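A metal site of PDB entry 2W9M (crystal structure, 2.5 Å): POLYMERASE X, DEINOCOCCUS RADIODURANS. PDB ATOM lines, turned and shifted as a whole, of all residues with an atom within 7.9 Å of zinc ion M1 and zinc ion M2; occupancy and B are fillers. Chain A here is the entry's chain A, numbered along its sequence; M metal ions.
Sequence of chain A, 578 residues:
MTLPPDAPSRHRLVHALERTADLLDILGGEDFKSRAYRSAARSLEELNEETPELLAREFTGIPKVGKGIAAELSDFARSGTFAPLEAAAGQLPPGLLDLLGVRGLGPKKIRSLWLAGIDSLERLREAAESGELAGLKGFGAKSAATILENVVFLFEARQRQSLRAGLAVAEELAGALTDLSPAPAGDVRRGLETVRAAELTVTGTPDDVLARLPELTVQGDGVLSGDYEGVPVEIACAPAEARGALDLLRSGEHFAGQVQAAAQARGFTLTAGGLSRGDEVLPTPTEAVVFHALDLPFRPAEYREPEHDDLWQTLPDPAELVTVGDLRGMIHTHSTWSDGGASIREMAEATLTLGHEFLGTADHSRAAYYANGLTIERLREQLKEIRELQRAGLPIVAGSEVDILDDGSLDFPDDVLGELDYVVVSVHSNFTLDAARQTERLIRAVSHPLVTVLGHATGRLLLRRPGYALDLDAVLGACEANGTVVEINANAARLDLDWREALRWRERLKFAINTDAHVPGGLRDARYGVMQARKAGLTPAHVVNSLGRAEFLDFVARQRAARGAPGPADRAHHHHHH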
ATOM      1  N   GLY A  90      38.012  36.376 -25.032  1.00  0.00           N
ATOM      2  CA  GLY A  90      36.607  36.241 -24.721  1.00  0.00           C
ATOM      3  C   GLY A  90      35.786  35.588 -25.822  1.00  0.00           C
ATOM      4  O   GLY A  90      34.654  35.148 -25.584  1.00  0.00           O
ATOM      5  N   GLN A  91      36.360  35.495 -27.013  1.00  0.00           N
ATOM      6  CA  GLN A  91      35.627  34.959 -28.169  1.00  0.00           C
ATOM      7  C   GLN A  91      36.024  33.534 -28.518  1.00  0.00           C
ATOM      8  O   GLN A  91      35.185  32.737 -28.932  1.00  0.00           O
ATOM      9  CB  GLN A  91      35.824  35.865 -29.376  1.00  0.00           C
ATOM     10  CG  GLN A  91      35.291  37.271 -29.174  1.00  0.00           C
ATOM     11  CD  GLN A  91      35.574  38.162 -30.346  1.00  0.00           C
ATOM     12  OE1 GLN A  91      35.787  37.684 -31.462  1.00  0.00           O
ATOM     13  NE2 GLN A  91      35.588  39.466 -30.117  1.00  0.00           N
ATOM     14  N   LEU A  92      37.310  33.229 -28.351  1.00  0.00           N
ATOM     15  CA  LEU A  92      37.835  31.924 -28.732  1.00  0.00           C
ATOM     16  C   LEU A  92      37.392  30.799 -27.799  1.00  0.00           C
ATOM     17  O   LEU A  92      37.124  31.040 -26.608  1.00  0.00           O
ATOM     18  CB  LEU A  92      39.365  31.980 -28.814  1.00  0.00           C
ATOM     19  CG  LEU A  92      39.894  32.847 -29.965  1.00  0.00           C
ATOM     20  CD1 LEU A  92      41.411  32.945 -29.902  1.00  0.00           C
ATOM     21  CD2 LEU A  92      39.448  32.309 -31.323  1.00  0.00           C
ATOM     22  N   PRO A  93      37.302  29.575 -28.327  1.00  0.00           N
ATOM     23  CA  PRO A  93      36.914  28.395 -27.548  1.00  0.00           C
ATOM     24  C   PRO A  93      37.970  28.096 -26.493  1.00  0.00           C
ATOM     25  O   PRO A  93      39.150  28.317 -26.735  1.00  0.00           O
ATOM     26  CB  PRO A  93      36.902  27.274 -28.591  1.00  0.00           C
ATOM     27  CG  PRO A  93      36.804  27.962 -29.913  1.00  0.00           C
ATOM     28  CD  PRO A  93      37.533  29.250 -29.740  1.00  0.00           C
ATOM     29  N   PRO A  94      37.545  27.568 -25.336  1.00  0.00           N
ATOM     30  CA  PRO A  94      38.442  27.247 -24.214  1.00  0.00           C
ATOM     31  C   PRO A  94      39.589  26.337 -24.625  1.00  0.00           C
ATOM     32  O   PRO A  94      40.724  26.559 -24.223  1.00  0.00           O
ATOM     33  CB  PRO A  94      37.517  26.501 -23.241  1.00  0.00           C
ATOM     34  CG  PRO A  94      36.165  27.034 -23.537  1.00  0.00           C
ATOM     35  CD  PRO A  94      36.142  27.268 -25.021  1.00  0.00           C
ATOM     36  N   HIS A 332      23.305  24.174 -30.485  1.00  0.00           N
ATOM     37  CA  HIS A 332      24.443  25.021 -30.180  1.00  0.00           C
ATOM     38  C   HIS A 332      25.767  24.325 -30.508  1.00  0.00           C
ATOM     39  O   HIS A 332      26.555  23.994 -29.635  1.00  0.00           O
ATOM     40  CB  HIS A 332      24.402  25.485 -28.726  1.00  0.00           C
ATOM     41  CG  HIS A 332      25.435  26.520 -28.396  1.00  0.00           C
ATOM     42  ND1 HIS A 332      25.741  26.878 -27.101  1.00  0.00           N
ATOM     43  CD2 HIS A 332      26.242  27.258 -29.189  1.00  0.00           C
ATOM     44  CE1 HIS A 332      26.682  27.798 -27.113  1.00  0.00           C
ATOM     45  NE2 HIS A 332      27.005  28.048 -28.373  1.00  0.00           N
ATOM     46  N   THR A 333      25.989  24.099 -31.800  1.00  0.00           N
ATOM     47  CA  THR A 333      27.238  23.524 -32.280  1.00  0.00           C
ATOM     48  C   THR A 333      27.875  24.500 -33.263  1.00  0.00           C
ATOM     49  O   THR A 333      27.184  25.345 -33.840  1.00  0.00           O
ATOM     50  CB  THR A 333      26.992  22.187 -32.992  1.00  0.00           C
ATOM     51  OG1 THR A 333      26.151  22.415 -34.130  1.00  0.00           O
ATOM     52  CG2 THR A 333      26.320  21.195 -32.063  1.00  0.00           C
ATOM     53  N   HIS A 334      29.183  24.396 -33.471  1.00  0.00           N
ATOM     54  CA  HIS A 334      29.885  25.301 -34.383  1.00  0.00           C
ATOM     55  C   HIS A 334      30.485  24.561 -35.578  1.00  0.00           C
ATOM     56  O   HIS A 334      30.849  23.391 -35.472  1.00  0.00           O
ATOM     57  CB  HIS A 334      30.953  26.105 -33.652  1.00  0.00           C
ATOM     58  CG  HIS A 334      30.395  27.054 -32.643  1.00  0.00           C
ATOM     59  ND1 HIS A 334      30.256  28.408 -32.881  1.00  0.00           N
ATOM     60  CD2 HIS A 334      29.919  26.848 -31.389  1.00  0.00           C
ATOM     61  CE1 HIS A 334      29.727  28.997 -31.827  1.00  0.00           C
ATOM     62  NE2 HIS A 334      29.510  28.060 -30.901  1.00  0.00           N
ATOM     63  N   SER A 338      32.164  29.352 -38.854  1.00  0.00           N
ATOM     64  CA  SER A 338      32.553  30.204 -37.747  1.00  0.00           C
ATOM     65  C   SER A 338      33.981  29.850 -37.306  1.00  0.00           C
ATOM     66  O   SER A 338      34.938  29.996 -38.075  1.00  0.00           O
ATOM     67  CB  SER A 338      31.589  30.016 -36.584  1.00  0.00           C
ATOM     68  OG  SER A 338      31.569  31.139 -35.730  1.00  0.00           O
ATOM     69  N   ASP A 339      34.114  29.393 -36.071  1.00  0.00           N
ATOM     70  CA  ASP A 339      35.404  28.953 -35.556  1.00  0.00           C
ATOM     71  C   ASP A 339      35.426  27.458 -35.236  1.00  0.00           C
ATOM     72  O   ASP A 339      36.182  27.011 -34.385  1.00  0.00           O
ATOM     73  CB  ASP A 339      35.813  29.778 -34.333  1.00  0.00           C
ATOM     74  CG  ASP A 339      34.870  29.596 -33.157  1.00  0.00           C
ATOM     75  OD1 ASP A 339      33.767  29.030 -33.349  1.00  0.00           O
ATOM     76  OD2 ASP A 339      35.226  30.016 -32.031  1.00  0.00           O
ATOM     77  N   ALA A 362      24.642  26.753 -34.855  1.00  0.00           N
ATOM     78  CA  ALA A 362      24.741  27.951 -34.015  1.00  0.00           C
ATOM     79  C   ALA A 362      26.129  28.611 -34.035  1.00  0.00           C
ATOM     80  O   ALA A 362      26.800  28.668 -33.014  1.00  0.00           O
ATOM     81  CB  ALA A 362      24.331  27.641 -32.585  1.00  0.00           C
ATOM     82  N   ASP A 363      26.529  29.101 -35.197  1.00  0.00           N
ATOM     83  CA  ASP A 363      27.824  29.773 -35.336  1.00  0.00           C
ATOM     84  C   ASP A 363      27.741  31.210 -34.828  1.00  0.00           C
ATOM     85  O   ASP A 363      26.654  31.760 -34.681  1.00  0.00           O
ATOM     86  CB  ASP A 363      28.291  29.717 -36.804  1.00  0.00           C
ATOM     87  CG  ASP A 363      28.816  28.341 -37.192  1.00  0.00           C
ATOM     88  OD1 ASP A 363      29.818  27.898 -36.601  1.00  0.00           O
ATOM     89  OD2 ASP A 363      28.212  27.697 -38.080  1.00  0.00           O
ATOM     90  N   HIS A 364      28.890  31.815 -34.546  1.00  0.00           N
ATOM     91  CA  HIS A 364      28.914  33.174 -33.997  1.00  0.00           C
ATOM     92  C   HIS A 364      28.472  34.187 -35.028  1.00  0.00           C
ATOM     93  O   HIS A 364      28.343  33.886 -36.219  1.00  0.00           O
ATOM     94  CB  HIS A 364      30.321  33.552 -33.519  1.00  0.00           C
ATOM     95  CG  HIS A 364      30.935  32.567 -32.588  1.00  0.00           C
ATOM     96  ND1 HIS A 364      30.751  32.610 -31.222  1.00  0.00           N
ATOM     97  CD2 HIS A 364      31.731  31.497 -32.834  1.00  0.00           C
ATOM     98  CE1 HIS A 364      31.412  31.608 -30.667  1.00  0.00           C
ATOM     99  NE2 HIS A 364      32.005  30.920 -31.618  1.00  0.00           N
ATOM    100  N   GLU A 401      24.513  31.817 -32.715  1.00  0.00           N
ATOM    101  CA  GLU A 401      24.866  32.308 -31.392  1.00  0.00           C
ATOM    102  C   GLU A 401      25.087  33.806 -31.481  1.00  0.00           C
ATOM    103  O   GLU A 401      26.189  34.271 -31.779  1.00  0.00           O
ATOM    104  CB  GLU A 401      26.105  31.616 -30.833  1.00  0.00           C
ATOM    105  CG  GLU A 401      26.353  31.974 -29.373  1.00  0.00           C
ATOM    106  CD  GLU A 401      27.579  31.330 -28.793  1.00  0.00           C
ATOM    107  OE1 GLU A 401      28.242  30.560 -29.527  1.00  0.00           O
ATOM    108  OE2 GLU A 401      27.878  31.598 -27.604  1.00  0.00           O
ATOM    109  N   VAL A 424      20.323  31.527 -30.018  1.00  0.00           N
ATOM    110  CA  VAL A 424      21.057  31.497 -28.752  1.00  0.00           C
ATOM    111  C   VAL A 424      21.687  32.866 -28.538  1.00  0.00           C
ATOM    112  O   VAL A 424      22.226  33.450 -29.471  1.00  0.00           O
ATOM    113  CB  VAL A 424      22.182  30.423 -28.767  1.00  0.00           C
ATOM    114  CG1 VAL A 424      22.980  30.450 -27.456  1.00  0.00           C
ATOM    115  CG2 VAL A 424      21.622  29.037 -29.022  1.00  0.00           C
ATOM    116  N   VAL A 425      21.600  33.395 -27.322  1.00  0.00           N
ATOM    117  CA  VAL A 425      22.283  34.643 -26.990  1.00  0.00           C
ATOM    118  C   VAL A 425      23.382  34.410 -25.972  1.00  0.00           C
ATOM    119  O   VAL A 425      23.254  33.566 -25.084  1.00  0.00           O
ATOM    120  CB  VAL A 425      21.311  35.730 -26.466  1.00  0.00           C
ATOM    121  CG1 VAL A 425      20.243  36.006 -27.506  1.00  0.00           C
ATOM    122  CG2 VAL A 425      20.697  35.297 -25.152  1.00  0.00           C
ATOM    123  N   SER A 426      24.474  35.157 -26.099  1.00  0.00           N
ATOM    124  CA  SER A 426      25.657  34.927 -25.277  1.00  0.00           C
ATOM    125  C   SER A 426      26.528  36.166 -25.167  1.00  0.00           C
ATOM    126  O   SER A 426      26.525  37.009 -26.051  1.00  0.00           O
ATOM    127  CB  SER A 426      26.490  33.784 -25.868  1.00  0.00           C
ATOM    128  OG  SER A 426      25.762  32.564 -25.874  1.00  0.00           O
ATOM    129  N   VAL A 427      27.275  36.251 -24.067  1.00  0.00           N
ATOM    130  CA  VAL A 427      28.278  37.290 -23.889  1.00  0.00           C
ATOM    131  C   VAL A 427      29.643  36.771 -24.336  1.00  0.00           C
ATOM    132  O   VAL A 427      30.068  35.688 -23.938  1.00  0.00           O
ATOM    133  CB  VAL A 427      28.374  37.729 -22.413  1.00  0.00           C
ATOM    134  CG1 VAL A 427      29.372  38.868 -22.269  1.00  0.00           C
ATOM    135  CG2 VAL A 427      27.014  38.151 -21.897  1.00  0.00           C
ATOM    136  N   HIS A 428      30.332  37.548 -25.173  1.00  0.00           N
ATOM    137  CA  HIS A 428      31.663  37.208 -25.635  1.00  0.00           C
ATOM    138  C   HIS A 428      32.567  38.447 -25.635  1.00  0.00           C
ATOM    139  O   HIS A 428      33.663  38.449 -26.215  1.00  0.00           O
ATOM    140  CB  HIS A 428      31.614  36.607 -27.038  1.00  0.00           C
ATOM    141  CG  HIS A 428      31.184  35.173 -27.072  1.00  0.00           C
ATOM    142  ND1 HIS A 428      31.946  34.155 -26.530  1.00  0.00           N
ATOM    143  CD2 HIS A 428      30.093  34.585 -27.603  1.00  0.00           C
ATOM    144  CE1 HIS A 428      31.322  33.004 -26.714  1.00  0.00           C
ATOM    145  NE2 HIS A 428      30.189  33.243 -27.356  1.00  0.00           N
ATOM    146  N   GLY A 455      23.016  31.283 -23.656  1.00  0.00           N
ATOM    147  CA  GLY A 455      24.254  30.515 -23.655  1.00  0.00           C
ATOM    148  C   GLY A 455      25.111  30.757 -22.415  1.00  0.00           C
ATOM    149  O   GLY A 455      25.079  31.849 -21.848  1.00  0.00           O
ATOM    150  N   HIS A 456      25.877  29.747 -22.010  1.00  0.00           N
ATOM    151  CA  HIS A 456      26.757  29.793 -20.826  1.00  0.00           C
ATOM    152  C   HIS A 456      26.616  31.060 -19.974  1.00  0.00           C
ATOM    153  O   HIS A 456      27.463  31.958 -20.038  1.00  0.00           O
ATOM    154  CB  HIS A 456      28.216  29.585 -21.230  1.00  0.00           C
ATOM    155  CG  HIS A 456      28.602  30.347 -22.458  1.00  0.00           C
ATOM    156  ND1 HIS A 456      28.840  31.709 -22.446  1.00  0.00           N
ATOM    157  CD2 HIS A 456      28.786  29.945 -23.733  1.00  0.00           C
ATOM    158  CE1 HIS A 456      29.159  32.105 -23.664  1.00  0.00           C
ATOM    159  NE2 HIS A 456      29.136  31.057 -24.468  1.00  0.00           N
ATOM    160  N   GLU A 487      20.961  27.599 -20.668  1.00  0.00           N
ATOM    161  CA  GLU A 487      21.845  26.536 -21.123  1.00  0.00           C
ATOM    162  C   GLU A 487      22.731  26.000 -20.000  1.00  0.00           C
ATOM    163  O   GLU A 487      23.236  26.758 -19.175  1.00  0.00           O
ATOM    164  CB  GLU A 487      22.722  27.037 -22.278  1.00  0.00           C
ATOM    165  CG  GLU A 487      23.919  26.152 -22.630  1.00  0.00           C
ATOM    166  CD  GLU A 487      24.645  26.635 -23.884  1.00  0.00           C
ATOM    167  OE1 GLU A 487      24.119  26.390 -24.995  1.00  0.00           O
ATOM    168  OE2 GLU A 487      25.735  27.238 -23.761  1.00  0.00           O
ATOM    169  N   ASN A 489      26.008  24.416 -20.322  1.00  0.00           N
ATOM    170  CA  ASN A 489      27.018  24.168 -21.335  1.00  0.00           C
ATOM    171  C   ASN A 489      27.860  22.974 -20.958  1.00  0.00           C
ATOM    172  O   ASN A 489      28.562  22.979 -19.949  1.00  0.00           O
ATOM    173  CB  ASN A 489      27.871  25.422 -21.533  1.00  0.00           C
ATOM    174  CG  ASN A 489      28.659  25.396 -22.830  1.00  0.00           C
ATOM    175  OD1 ASN A 489      29.551  24.570 -23.003  1.00  0.00           O
ATOM    176  ND2 ASN A 489      28.336  26.311 -23.733  1.00  0.00           N
ATOM    177  N   ARG A 494      33.536  24.763 -19.254  1.00  0.00           N
ATOM    178  CA  ARG A 494      32.475  25.682 -18.875  1.00  0.00           C
ATOM    179  C   ARG A 494      31.585  25.130 -17.762  1.00  0.00           C
ATOM    180  O   ARG A 494      31.549  25.680 -16.664  1.00  0.00           O
ATOM    181  CB  ARG A 494      31.640  26.091 -20.094  1.00  0.00           C
ATOM    182  CG  ARG A 494      32.414  26.934 -21.084  1.00  0.00           C
ATOM    183  CD  ARG A 494      31.535  27.337 -22.261  1.00  0.00           C
ATOM    184  NE  ARG A 494      32.286  28.049 -23.296  1.00  0.00           N
ATOM    185  CZ  ARG A 494      32.620  29.329 -23.223  1.00  0.00           C
ATOM    186  NH1 ARG A 494      32.293  30.054 -22.161  1.00  0.00           N
ATOM    187  NH2 ARG A 494      33.296  29.885 -24.223  1.00  0.00           N
ATOM    188  N   THR A 515      26.448  21.006 -25.988  1.00  0.00           N
ATOM    189  CA  THR A 515      27.869  20.676 -25.997  1.00  0.00           C
ATOM    190  C   THR A 515      28.753  21.863 -26.423  1.00  0.00           C
ATOM    191  O   THR A 515      29.923  21.931 -26.037  1.00  0.00           O
ATOM    192  CB  THR A 515      28.139  19.503 -26.953  1.00  0.00           C
ATOM    193  OG1 THR A 515      27.704  19.857 -28.265  1.00  0.00           O
ATOM    194  CG2 THR A 515      27.402  18.266 -26.494  1.00  0.00           C
ATOM    195  N   ASP A 516      28.193  22.773 -27.211  1.00  0.00           N
ATOM    196  CA  ASP A 516      28.975  23.874 -27.776  1.00  0.00           C
ATOM    197  C   ASP A 516      30.150  23.321 -28.573  1.00  0.00           C
ATOM    198  O   ASP A 516      31.232  23.902 -28.588  1.00  0.00           O
ATOM    199  CB  ASP A 516      29.472  24.798 -26.663  1.00  0.00           C
ATOM    200  CG  ASP A 516      29.816  26.189 -27.167  1.00  0.00           C
ATOM    201  OD1 ASP A 516      29.788  26.389 -28.394  1.00  0.00           O
ATOM    202  OD2 ASP A 516      30.111  27.075 -26.335  1.00  0.00           O
ATOM    203  N   ALA A 517      29.925  22.202 -29.254  1.00  0.00           N
ATOM    204  CA  ALA A 517      30.977  21.518 -30.013  1.00  0.00           C
ATOM    205  C   ALA A 517      31.579  22.372 -31.131  1.00  0.00           C
ATOM    206  O   ALA A 517      30.863  22.908 -31.985  1.00  0.00           O
ATOM    207  CB  ALA A 517      30.451  20.205 -30.585  1.00  0.00           C
ATOM    208  N   HIS A 518      32.902  22.500 -31.136  1.00  0.00           N
ATOM    209  CA  HIS A 518      33.604  23.173 -32.210  1.00  0.00           C
ATOM    210  C   HIS A 518      34.265  22.158 -33.147  1.00  0.00           C
ATOM    211  O   HIS A 518      34.953  22.518 -34.095  1.00  0.00           O
ATOM    212  CB  HIS A 518      34.647  24.136 -31.644  1.00  0.00           C
ATOM    213  CG  HIS A 518      34.059  25.391 -31.094  1.00  0.00           C
ATOM    214  ND1 HIS A 518      33.363  25.433 -29.907  1.00  0.00           N
ATOM    215  CD2 HIS A 518      34.037  26.654 -31.577  1.00  0.00           C
ATOM    216  CE1 HIS A 518      32.948  26.658 -29.674  1.00  0.00           C
ATOM    217  NE2 HIS A 518      33.341  27.433 -30.679  1.00  0.00           N
HETATM  218 ZN    ZN M   1      29.721  30.911 -26.818  1.00  0.00          ZN
HETATM  219 ZN    ZN M   2      29.154  28.684 -28.720  1.00  0.00          ZN
HETATM  220 ZN    ZN M   3      33.322  29.515 -30.869  1.00  0.00          ZN
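N of Glu 401 lies within hydrogen-bond range of O of Asp 363 (2.9 Å).
The backbone NH (N) of His 334 lies within hydrogen-bond range of the backbone carbonyl oxygen (O) of Ala 517, 2.7 Å away.
The backbone carbonyl oxygen (O) of Gly 90 lies within hydrogen-bond range of a ring nitrogen (ND1) of His 428 (3.0 Å).
OD2 of Asp 516 is in salt-bridge range of NE of Arg 494.
The side-chain carboxylate of Glu 401 lies close to the side-chain hydroxyl of Ser 426, at 2.9 Å.
OD2 of Asp 516 lies within hydrogen-bond range of ND2 of Asn 489, 3.2 Å away.
ND1 of His 334 lies close to O of Ala 362 (3.5 Å).
A ring nitrogen (ND1) of His 518 lies within hydrogen-bond range of the backbone carbonyl oxygen of Asp 516 (2.9 Å).
Within 4 Å of zinc ion M1: Glu 401, His 428, His 456 and Asp 516.
The nearest printed residue that does not touch zinc ion M1 is His 332 (4.2 Å).
Within 4 Å of zinc ion M2: His 332, His 334, Glu 401 and Asp 516.
The nearest printed residue that does not touch zinc ion M2 is His 364 (4.2 Å).
Zinc ion M1 is bound by OE2 of Glu 401 (2.1 Å), NE2 of His 456 (2.4 Å) and NE2 of His 428 (2.4 Å).
Zinc ion M2 is bound by the side-chain carboxylate (OE1) of Glu 401, 2.2 Å away.
Zinc ion M2 is bound by a ring nitrogen (NE2) of His 332 (2.3 Å).
Zinc ion M2 is bound by NE2 of His 334, at 2.3 Å.
The side-chain carboxylate (OD1) of Asp 516 binds zinc ion M2, at 2.4 Å.
Zinc ion M2 has four donor atoms within binding distance.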
